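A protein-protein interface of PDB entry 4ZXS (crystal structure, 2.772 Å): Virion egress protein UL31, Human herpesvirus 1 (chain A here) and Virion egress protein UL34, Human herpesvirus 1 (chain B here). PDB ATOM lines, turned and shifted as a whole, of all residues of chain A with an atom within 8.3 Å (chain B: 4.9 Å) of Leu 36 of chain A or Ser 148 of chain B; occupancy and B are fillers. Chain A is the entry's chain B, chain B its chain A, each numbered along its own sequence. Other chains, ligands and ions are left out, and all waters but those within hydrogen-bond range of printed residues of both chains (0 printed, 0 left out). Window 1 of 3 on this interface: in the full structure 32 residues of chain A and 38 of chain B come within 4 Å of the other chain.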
ATOM      1  N   TYR A  15       9.247  -4.632  -1.253  1.00  0.00           N
ATOM      2  CA  TYR A  15       8.225  -5.224  -0.395  1.00  0.00           C
ATOM      3  C   TYR A  15       8.231  -4.626   1.008  1.00  0.00           C
ATOM      4  O   TYR A  15       7.235  -4.713   1.728  1.00  0.00           O
ATOM      5  CB  TYR A  15       8.413  -6.740  -0.308  1.00  0.00           C
ATOM      6  CG  TYR A  15       7.977  -7.484  -1.549  1.00  0.00           C
ATOM      7  CD1 TYR A  15       6.645  -7.821  -1.751  1.00  0.00           C
ATOM      8  CD2 TYR A  15       8.901  -7.863  -2.512  1.00  0.00           C
ATOM      9  CE1 TYR A  15       6.244  -8.502  -2.885  1.00  0.00           C
ATOM     10  CE2 TYR A  15       8.511  -8.542  -3.651  1.00  0.00           C
ATOM     11  CZ  TYR A  15       7.181  -8.862  -3.831  1.00  0.00           C
ATOM     12  OH  TYR A  15       6.789  -9.542  -4.961  1.00  0.00           O
ATOM     13  N   GLU A  29      -4.506  -7.323   5.107  1.00  0.00           N
ATOM     14  CA  GLU A  29      -3.504  -8.291   4.686  1.00  0.00           C
ATOM     15  C   GLU A  29      -4.149  -9.644   4.405  1.00  0.00           C
ATOM     16  O   GLU A  29      -3.849 -10.282   3.399  1.00  0.00           O
ATOM     17  CB  GLU A  29      -2.412  -8.430   5.750  1.00  0.00           C
ATOM     18  CG  GLU A  29      -1.501  -9.631   5.557  1.00  0.00           C
ATOM     19  CD  GLU A  29      -0.202  -9.505   6.327  1.00  0.00           C
ATOM     20  OE1 GLU A  29      -0.249  -9.479   7.576  1.00  0.00           O
ATOM     21  OE2 GLU A  29       0.869  -9.435   5.687  1.00  0.00           O
ATOM     22  N   ILE A  30      -5.044 -10.069   5.294  1.00  0.00           N
ATOM     23  CA  ILE A  30      -5.754 -11.334   5.116  1.00  0.00           C
ATOM     24  C   ILE A  30      -6.575 -11.334   3.828  1.00  0.00           C
ATOM     25  O   ILE A  30      -6.551 -12.304   3.062  1.00  0.00           O
ATOM     26  CB  ILE A  30      -6.691 -11.628   6.309  1.00  0.00           C
ATOM     27  CG1 ILE A  30      -5.895 -11.673   7.615  1.00  0.00           C
ATOM     28  CG2 ILE A  30      -7.432 -12.938   6.098  1.00  0.00           C
ATOM     29  CD1 ILE A  30      -6.707 -12.128   8.811  1.00  0.00           C
ATOM     30  N   ALA A  31      -7.282 -10.234   3.583  1.00  0.00           N
ATOM     31  CA  ALA A  31      -8.082 -10.095   2.370  1.00  0.00           C
ATOM     32  C   ALA A  31      -7.212 -10.163   1.115  1.00  0.00           C
ATOM     33  O   ALA A  31      -7.547 -10.853   0.146  1.00  0.00           O
ATOM     34  CB  ALA A  31      -8.866  -8.793   2.401  1.00  0.00           C
ATOM     35  N   ILE A  32      -6.085  -9.455   1.149  1.00  0.00           N
ATOM     36  CA  ILE A  32      -5.157  -9.422   0.023  1.00  0.00           C
ATOM     37  C   ILE A  32      -4.588 -10.813  -0.250  1.00  0.00           C
ATOM     38  O   ILE A  32      -4.468 -11.229  -1.403  1.00  0.00           O
ATOM     39  CB  ILE A  32      -4.004  -8.425   0.273  1.00  0.00           C
ATOM     40  CG1 ILE A  32      -4.531  -6.989   0.258  1.00  0.00           C
ATOM     41  CG2 ILE A  32      -2.915  -8.582  -0.772  1.00  0.00           C
ATOM     42  CD1 ILE A  32      -3.523  -5.964   0.723  1.00  0.00           C
ATOM     43  N   VAL A  33      -4.250 -11.533   0.816  1.00  0.00           N
ATOM     44  CA  VAL A  33      -3.741 -12.894   0.691  1.00  0.00           C
ATOM     45  C   VAL A  33      -4.792 -13.808   0.065  1.00  0.00           C
ATOM     46  O   VAL A  33      -4.486 -14.599  -0.828  1.00  0.00           O
ATOM     47  CB  VAL A  33      -3.306 -13.465   2.058  1.00  0.00           C
ATOM     48  CG1 VAL A  33      -3.063 -14.965   1.964  1.00  0.00           C
ATOM     49  CG2 VAL A  33      -2.062 -12.750   2.563  1.00  0.00           C
ATOM     50  N   ARG A  34      -6.034 -13.687   0.525  1.00  0.00           N
ATOM     51  CA  ARG A  34      -7.119 -14.507  -0.009  1.00  0.00           C
ATOM     52  C   ARG A  34      -7.455 -14.168  -1.462  1.00  0.00           C
ATOM     53  O   ARG A  34      -7.988 -15.005  -2.191  1.00  0.00           O
ATOM     54  CB  ARG A  34      -8.374 -14.362   0.854  1.00  0.00           C
ATOM     55  CG  ARG A  34      -8.230 -14.906   2.265  1.00  0.00           C
ATOM     56  CD  ARG A  34      -9.542 -14.818   3.027  1.00  0.00           C
ATOM     57  NE  ARG A  34      -9.358 -15.049   4.457  1.00  0.00           N
ATOM     58  CZ  ARG A  34      -9.384 -16.248   5.031  1.00  0.00           C
ATOM     59  NH1 ARG A  34      -9.587 -17.333   4.298  1.00  0.00           N
ATOM     60  NH2 ARG A  34      -9.205 -16.360   6.340  1.00  0.00           N
ATOM     61  N   SER A  35      -7.148 -12.941  -1.877  1.00  0.00           N
ATOM     62  CA  SER A  35      -7.493 -12.473  -3.221  1.00  0.00           C
ATOM     63  C   SER A  35      -6.839 -13.265  -4.360  1.00  0.00           C
ATOM     64  O   SER A  35      -7.412 -13.386  -5.444  1.00  0.00           O
ATOM     65  CB  SER A  35      -7.128 -10.994  -3.364  1.00  0.00           C
ATOM     66  OG  SER A  35      -5.730 -10.801  -3.234  1.00  0.00           O
ATOM     67  N   LEU A  36      -5.646 -13.800  -4.117  1.00  0.00           N
ATOM     68  CA  LEU A  36      -4.877 -14.485  -5.158  1.00  0.00           C
ATOM     69  C   LEU A  36      -5.443 -15.863  -5.507  1.00  0.00           C
ATOM     70  O   LEU A  36      -4.885 -16.888  -5.115  1.00  0.00           O
ATOM     71  CB  LEU A  36      -3.415 -14.618  -4.727  1.00  0.00           C
ATOM     72  CG  LEU A  36      -2.742 -13.323  -4.268  1.00  0.00           C
ATOM     73  CD1 LEU A  36      -1.765 -13.592  -3.135  1.00  0.00           C
ATOM     74  CD2 LEU A  36      -2.044 -12.635  -5.432  1.00  0.00           C
ATOM     75  N   SER A  37      -6.550 -15.880  -6.245  1.00  0.00           N
ATOM     76  CA  SER A  37      -7.260 -17.121  -6.550  1.00  0.00           C
ATOM     77  C   SER A  37      -6.958 -17.699  -7.939  1.00  0.00           C
ATOM     78  O   SER A  37      -7.086 -18.904  -8.150  1.00  0.00           O
ATOM     79  CB  SER A  37      -8.769 -16.903  -6.411  1.00  0.00           C
ATOM     80  OG  SER A  37      -9.216 -15.861  -7.259  1.00  0.00           O
ATOM     81  N   VAL A  38      -6.583 -16.844  -8.886  1.00  0.00           N
ATOM     82  CA  VAL A  38      -6.356 -17.283 -10.263  1.00  0.00           C
ATOM     83  C   VAL A  38      -4.873 -17.531 -10.564  1.00  0.00           C
ATOM     84  O   VAL A  38      -4.031 -16.667 -10.326  1.00  0.00           O
ATOM     85  CB  VAL A  38      -6.924 -16.257 -11.275  1.00  0.00           C
ATOM     86  CG1 VAL A  38      -6.554 -14.837 -10.871  1.00  0.00           C
ATOM     87  CG2 VAL A  38      -6.448 -16.566 -12.690  1.00  0.00           C
ATOM     88  N   PRO A  39      -4.552 -18.728 -11.086  1.00  0.00           N
ATOM     89  CA  PRO A  39      -3.174 -19.112 -11.418  1.00  0.00           C
ATOM     90  C   PRO A  39      -2.695 -18.527 -12.747  1.00  0.00           C
ATOM     91  O   PRO A  39      -3.409 -18.591 -13.747  1.00  0.00           O
ATOM     92  CB  PRO A  39      -3.247 -20.638 -11.490  1.00  0.00           C
ATOM     93  CG  PRO A  39      -4.646 -20.925 -11.892  1.00  0.00           C
ATOM     94  CD  PRO A  39      -5.506 -19.827 -11.319  1.00  0.00           C
ATOM     95  N   LEU A  40      -1.493 -17.961 -12.743  1.00  0.00           N
ATOM     96  CA  LEU A  40      -0.937 -17.298 -13.919  1.00  0.00           C
ATOM     97  C   LEU A  40      -0.430 -18.265 -14.992  1.00  0.00           C
ATOM     98  O   LEU A  40      -0.421 -17.933 -16.178  1.00  0.00           O
ATOM     99  CB  LEU A  40       0.194 -16.359 -13.495  1.00  0.00           C
ATOM    100  CG  LEU A  40      -0.214 -15.312 -12.458  1.00  0.00           C
ATOM    101  CD1 LEU A  40       0.953 -14.404 -12.108  1.00  0.00           C
ATOM    102  CD2 LEU A  40      -1.400 -14.503 -12.960  1.00  0.00           C
ATOM    103  N   GLU B  65       5.599 -17.970  -0.873  1.00  0.00           N
ATOM    104  CA  GLU B  65       6.248 -16.713  -1.242  1.00  0.00           C
ATOM    105  C   GLU B  65       6.005 -15.617  -0.215  1.00  0.00           C
ATOM    106  O   GLU B  65       6.948 -14.994   0.266  1.00  0.00           O
ATOM    107  CB  GLU B  65       5.769 -16.237  -2.616  1.00  0.00           C
ATOM    108  CG  GLU B  65       6.246 -14.830  -2.960  1.00  0.00           C
ATOM    109  CD  GLU B  65       6.193 -14.527  -4.444  1.00  0.00           C
ATOM    110  OE1 GLU B  65       5.851 -15.437  -5.230  1.00  0.00           O
ATOM    111  OE2 GLU B  65       6.494 -13.376  -4.824  1.00  0.00           O
ATOM    112  N   TYR B  66       4.737 -15.388   0.114  1.00  0.00           N
ATOM    113  CA  TYR B  66       4.353 -14.335   1.049  1.00  0.00           C
ATOM    114  C   TYR B  66       5.061 -14.497   2.389  1.00  0.00           C
ATOM    115  O   TYR B  66       5.569 -13.528   2.960  1.00  0.00           O
ATOM    116  CB  TYR B  66       2.836 -14.337   1.257  1.00  0.00           C
ATOM    117  CG  TYR B  66       2.284 -13.036   1.792  1.00  0.00           C
ATOM    118  CD1 TYR B  66       2.346 -12.736   3.148  1.00  0.00           C
ATOM    119  CD2 TYR B  66       1.700 -12.106   0.943  1.00  0.00           C
ATOM    120  CE1 TYR B  66       1.844 -11.546   3.639  1.00  0.00           C
ATOM    121  CE2 TYR B  66       1.194 -10.916   1.427  1.00  0.00           C
ATOM    122  CZ  TYR B  66       1.269 -10.641   2.775  1.00  0.00           C
ATOM    123  OH  TYR B  66       0.766  -9.455   3.257  1.00  0.00           O
ATOM    124  N   MET B 145       2.570  -8.167  -5.004  1.00  0.00           N
ATOM    125  CA  MET B 145       1.212  -8.708  -4.889  1.00  0.00           C
ATOM    126  C   MET B 145       0.533  -8.949  -6.236  1.00  0.00           C
ATOM    127  O   MET B 145      -0.644  -9.309  -6.287  1.00  0.00           O
ATOM    128  CB  MET B 145       0.335  -7.797  -4.021  1.00  0.00           C
ATOM    129  CG  MET B 145       0.777  -7.717  -2.570  1.00  0.00           C
ATOM    130  SD  MET B 145       1.528  -9.247  -1.974  1.00  0.00           S
ATOM    131  CE  MET B 145       0.102 -10.328  -1.882  1.00  0.00           C
ATOM    132  N   MET B 146       1.271  -8.752  -7.322  1.00  0.00           N
ATOM    133  CA  MET B 146       0.753  -9.047  -8.652  1.00  0.00           C
ATOM    134  C   MET B 146       1.003 -10.509  -9.003  1.00  0.00           C
ATOM    135  O   MET B 146       0.361 -11.068  -9.892  1.00  0.00           O
ATOM    136  CB  MET B 146       1.380  -8.127  -9.698  1.00  0.00           C
ATOM    137  CG  MET B 146       0.990  -6.659  -9.565  1.00  0.00           C
ATOM    138  SD  MET B 146      -0.794  -6.371  -9.616  1.00  0.00           S
ATOM    139  CE  MET B 146      -1.177  -6.180  -7.873  1.00  0.00           C
ATOM    140  N   ALA B 147       1.956 -11.120  -8.304  1.00  0.00           N
ATOM    141  CA  ALA B 147       2.219 -12.547  -8.447  1.00  0.00           C
ATOM    142  C   ALA B 147       2.779 -13.126  -7.151  1.00  0.00           C
ATOM    143  O   ALA B 147       3.815 -12.677  -6.659  1.00  0.00           O
ATOM    144  CB  ALA B 147       3.176 -12.799  -9.601  1.00  0.00           C
ATOM    145  N   SER B 148       2.093 -14.128  -6.609  1.00  0.00           N
ATOM    146  CA  SER B 148       2.528 -14.778  -5.378  1.00  0.00           C
ATOM    147  C   SER B 148       2.380 -16.291  -5.494  1.00  0.00           C
ATOM    148  O   SER B 148       1.289 -16.797  -5.763  1.00  0.00           O
ATOM    149  CB  SER B 148       1.731 -14.252  -4.183  1.00  0.00           C
ATOM    150  OG  SER B 148       2.245 -14.757  -2.963  1.00  0.00           O
ATOM    151  N   MET B 149       3.478 -17.012  -5.289  1.00  0.00           N
ATOM    152  CA  MET B 149       3.465 -18.462  -5.436  1.00  0.00           C
ATOM    153  C   MET B 149       2.817 -19.154  -4.241  1.00  0.00           C
ATOM    154  O   MET B 149       3.054 -18.795  -3.088  1.00  0.00           O
ATOM    155  CB  MET B 149       4.884 -19.001  -5.637  1.00  0.00           C
ATOM    156  CG  MET B 149       4.928 -20.494  -5.943  1.00  0.00           C
ATOM    157  SD  MET B 149       6.579 -21.112  -6.318  1.00  0.00           S
ATOM    158  CE  MET B 149       7.102 -21.641  -4.691  1.00  0.00           C
ATOM    159  N   TRP B 150       1.988 -20.148  -4.542  1.00  0.00           N
ATOM    160  CA  TRP B 150       1.378 -21.004  -3.537  1.00  0.00           C
ATOM    161  C   TRP B 150       1.776 -22.452  -3.789  1.00  0.00           C
ATOM    162  O   TRP B 150       2.046 -22.844  -4.927  1.00  0.00           O
ATOM    163  CB  TRP B 150      -0.146 -20.870  -3.556  1.00  0.00           C
ATOM    164  CG  TRP B 150      -0.663 -19.572  -3.023  1.00  0.00           C
ATOM    165  CD1 TRP B 150      -0.554 -18.343  -3.604  1.00  0.00           C
ATOM    166  CD2 TRP B 150      -1.403 -19.379  -1.811  1.00  0.00           C
ATOM    167  NE1 TRP B 150      -1.164 -17.393  -2.821  1.00  0.00           N
ATOM    168  CE2 TRP B 150      -1.693 -18.003  -1.715  1.00  0.00           C
ATOM    169  CE3 TRP B 150      -1.840 -20.234  -0.795  1.00  0.00           C
ATOM    170  CZ2 TRP B 150      -2.402 -17.464  -0.644  1.00  0.00           C
ATOM    171  CZ3 TRP B 150      -2.543 -19.696   0.268  1.00  0.00           C
ATOM    172  CH2 TRP B 150      -2.817 -18.324   0.336  1.00  0.00           C
ATOM    173  N   ARG B 165       2.650 -23.305  -7.739  1.00  0.00           N
ATOM    174  CA  ARG B 165       2.009 -22.489  -8.768  1.00  0.00           C
ATOM    175  C   ARG B 165       1.947 -21.009  -8.409  1.00  0.00           C
ATOM    176  O   ARG B 165       1.486 -20.647  -7.329  1.00  0.00           O
ATOM    177  CB  ARG B 165       0.594 -23.004  -9.034  1.00  0.00           C
ATOM    178  CG  ARG B 165       0.481 -24.513  -9.033  1.00  0.00           C
ATOM    179  CD  ARG B 165      -0.968 -24.956  -9.019  1.00  0.00           C
ATOM    180  NE  ARG B 165      -1.130 -26.289  -9.589  1.00  0.00           N
ATOM    181  CZ  ARG B 165      -2.240 -27.013  -9.488  1.00  0.00           C
ATOM    182  NH1 ARG B 165      -3.287 -26.533  -8.831  1.00  0.00           N
ATOM    183  NH2 ARG B 165      -2.301 -28.217 -10.039  1.00  0.00           N
ATOM    184  N   PHE B 166       2.391 -20.155  -9.326  1.00  0.00           N
ATOM    185  CA  PHE B 166       2.247 -18.714  -9.153  1.00  0.00           C
ATOM    186  C   PHE B 166       0.795 -18.287  -9.342  1.00  0.00           C
ATOM    187  O   PHE B 166       0.196 -18.529 -10.390  1.00  0.00           O
ATOM    188  CB  PHE B 166       3.145 -17.955 -10.132  1.00  0.00           C
ATOM    189  CG  PHE B 166       4.602 -17.979  -9.766  1.00  0.00           C
ATOM    190  CD1 PHE B 166       5.087 -17.175  -8.748  1.00  0.00           C
ATOM    191  CD2 PHE B 166       5.489 -18.795 -10.450  1.00  0.00           C
ATOM    192  CE1 PHE B 166       6.427 -17.191  -8.411  1.00  0.00           C
ATOM    193  CE2 PHE B 166       6.831 -18.816 -10.118  1.00  0.00           C
ATOM    194  CZ  PHE B 166       7.300 -18.012  -9.097  1.00  0.00           C
ATOM    195  N   MET B 167       0.234 -17.655  -8.318  1.00  0.00           N
ATOM    196  CA  MET B 167      -1.147 -17.189  -8.354  1.00  0.00           C
ATOM    197  C   MET B 167      -1.199 -15.671  -8.468  1.00  0.00           C
ATOM    198  O   MET B 167      -0.356 -14.972  -7.908  1.00  0.00           O
ATOM    199  CB  MET B 167      -1.904 -17.651  -7.108  1.00  0.00           C
ATOM    200  CG  MET B 167      -1.760 -19.134  -6.807  1.00  0.00           C
ATOM    201  SD  MET B 167      -2.740 -20.158  -7.918  1.00  0.00           S
ATOM    202  CE  MET B 167      -4.335 -20.082  -7.109  1.00  0.00           C
ATOM    203  N   GLY B 168      -2.195 -15.166  -9.187  1.00  0.00           N
ATOM    204  CA  GLY B 168      -2.332 -13.736  -9.382  1.00  0.00           C
ATOM    205  C   GLY B 168      -3.612 -13.196  -8.778  1.00  0.00           C
ATOM    206  O   GLY B 168      -4.515 -13.963  -8.441  1.00  0.00           O
ATOM    207  N   PRO B 169      -3.696 -11.867  -8.631  1.00  0.00           N
ATOM    208  CA  PRO B 169      -4.868 -11.182  -8.080  1.00  0.00           C
ATOM    209  C   PRO B 169      -6.080 -11.257  -9.000  1.00  0.00           C
ATOM    210  O   PRO B 169      -5.941 -11.501 -10.198  1.00  0.00           O
ATOM    211  CB  PRO B 169      -4.391  -9.736  -7.930  1.00  0.00           C
ATOM    212  CG  PRO B 169      -3.349  -9.587  -8.973  1.00  0.00           C
ATOM    213  CD  PRO B 169      -2.645 -10.914  -9.026  1.00  0.00           C
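The side-chain hydroxyl (OH) of Tyr 66 of chain B is in hydrogen-bond range of the side-chain carboxylate (OE2) of Glu 29 of chain A (2.4 Å). The backbone carbonyl oxygen of Phe 166 of chain B lies within hydrogen-bond range of the backbone NH of Leu 40 of chain A (3.0 Å). N of Gly 168 of chain B sits at hydrogen-bond distance from O of Val 38 of chain A, 2.6 Å away.
The backbone NH (N) of Met 149 of chain B lies within hydrogen-bond range of the side-chain carboxylate (OE1) of Glu 65 of chain B, at 2.8 Å. The backbone carbonyl oxygen (O) of Ser 148 of chain B lies within hydrogen-bond range of the backbone NH (N) of Met 167 of chain B (2.9 Å). O of Arg 165 of chain B is in hydrogen-bond range of N of Trp 150 of chain B (2.9 Å).
Among the printed residues, pairs that only touch across the chains: Tyr 15 of chain A with Glu 65 of chain B, Ile 32 of chain A with Met 145 of chain B, Val 33 of chain A with Tyr 66 of chain B, Val 33 of chain A with Trp 150 of chain B, Leu 36 of chain A with Met 145 of chain B, Leu 36 of chain A with Ser 148 of chain B, Leu 36 of chain A with Trp 150 of chain B, Leu 36 of chain A with Met 167 of chain B, Leu 36 of chain A with Gly 168 of chain B, Leu 36 of chain A with Pro 169 of chain B, Ser 37 of chain A with Met 167 of chain B, Ser 37 of chain A with Gly 168 of chain B, Val 38 of chain A with Met 167 of chain B, Val 38 of chain A with Pro 169 of chain B, Pro 39 of chain A with Phe 166 of chain B, Pro 39 of chain A with Met 167 of chain B, Leu 40 of chain A with Ala 147 of chain B and Leu 40 of chain A with Gly 168 of chain B.
Printed residues of chain B within 4 Å of Ser 37 of chain A: Met 167 and Gly 168. Of chain A, only Leu 40 (3.7 Å) comes within 4 Å of Ala 147 of chain B. Of the printed residues of chain A, Ser 148 of chain B touches Leu 36 (3.7 Å). Printed residues of chain A within 4 Å of Pro 169 of chain B: Leu 36 and Val 38. The nearest printed residue of chain A that does not touch Trp 150 of chain B is Arg 34 of chain A (5.4 Å).
Among the printed residues, no Asp or Glu carboxylate lies within 4 Å of a Lys or Arg side-chain nitrogen of the other chain.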
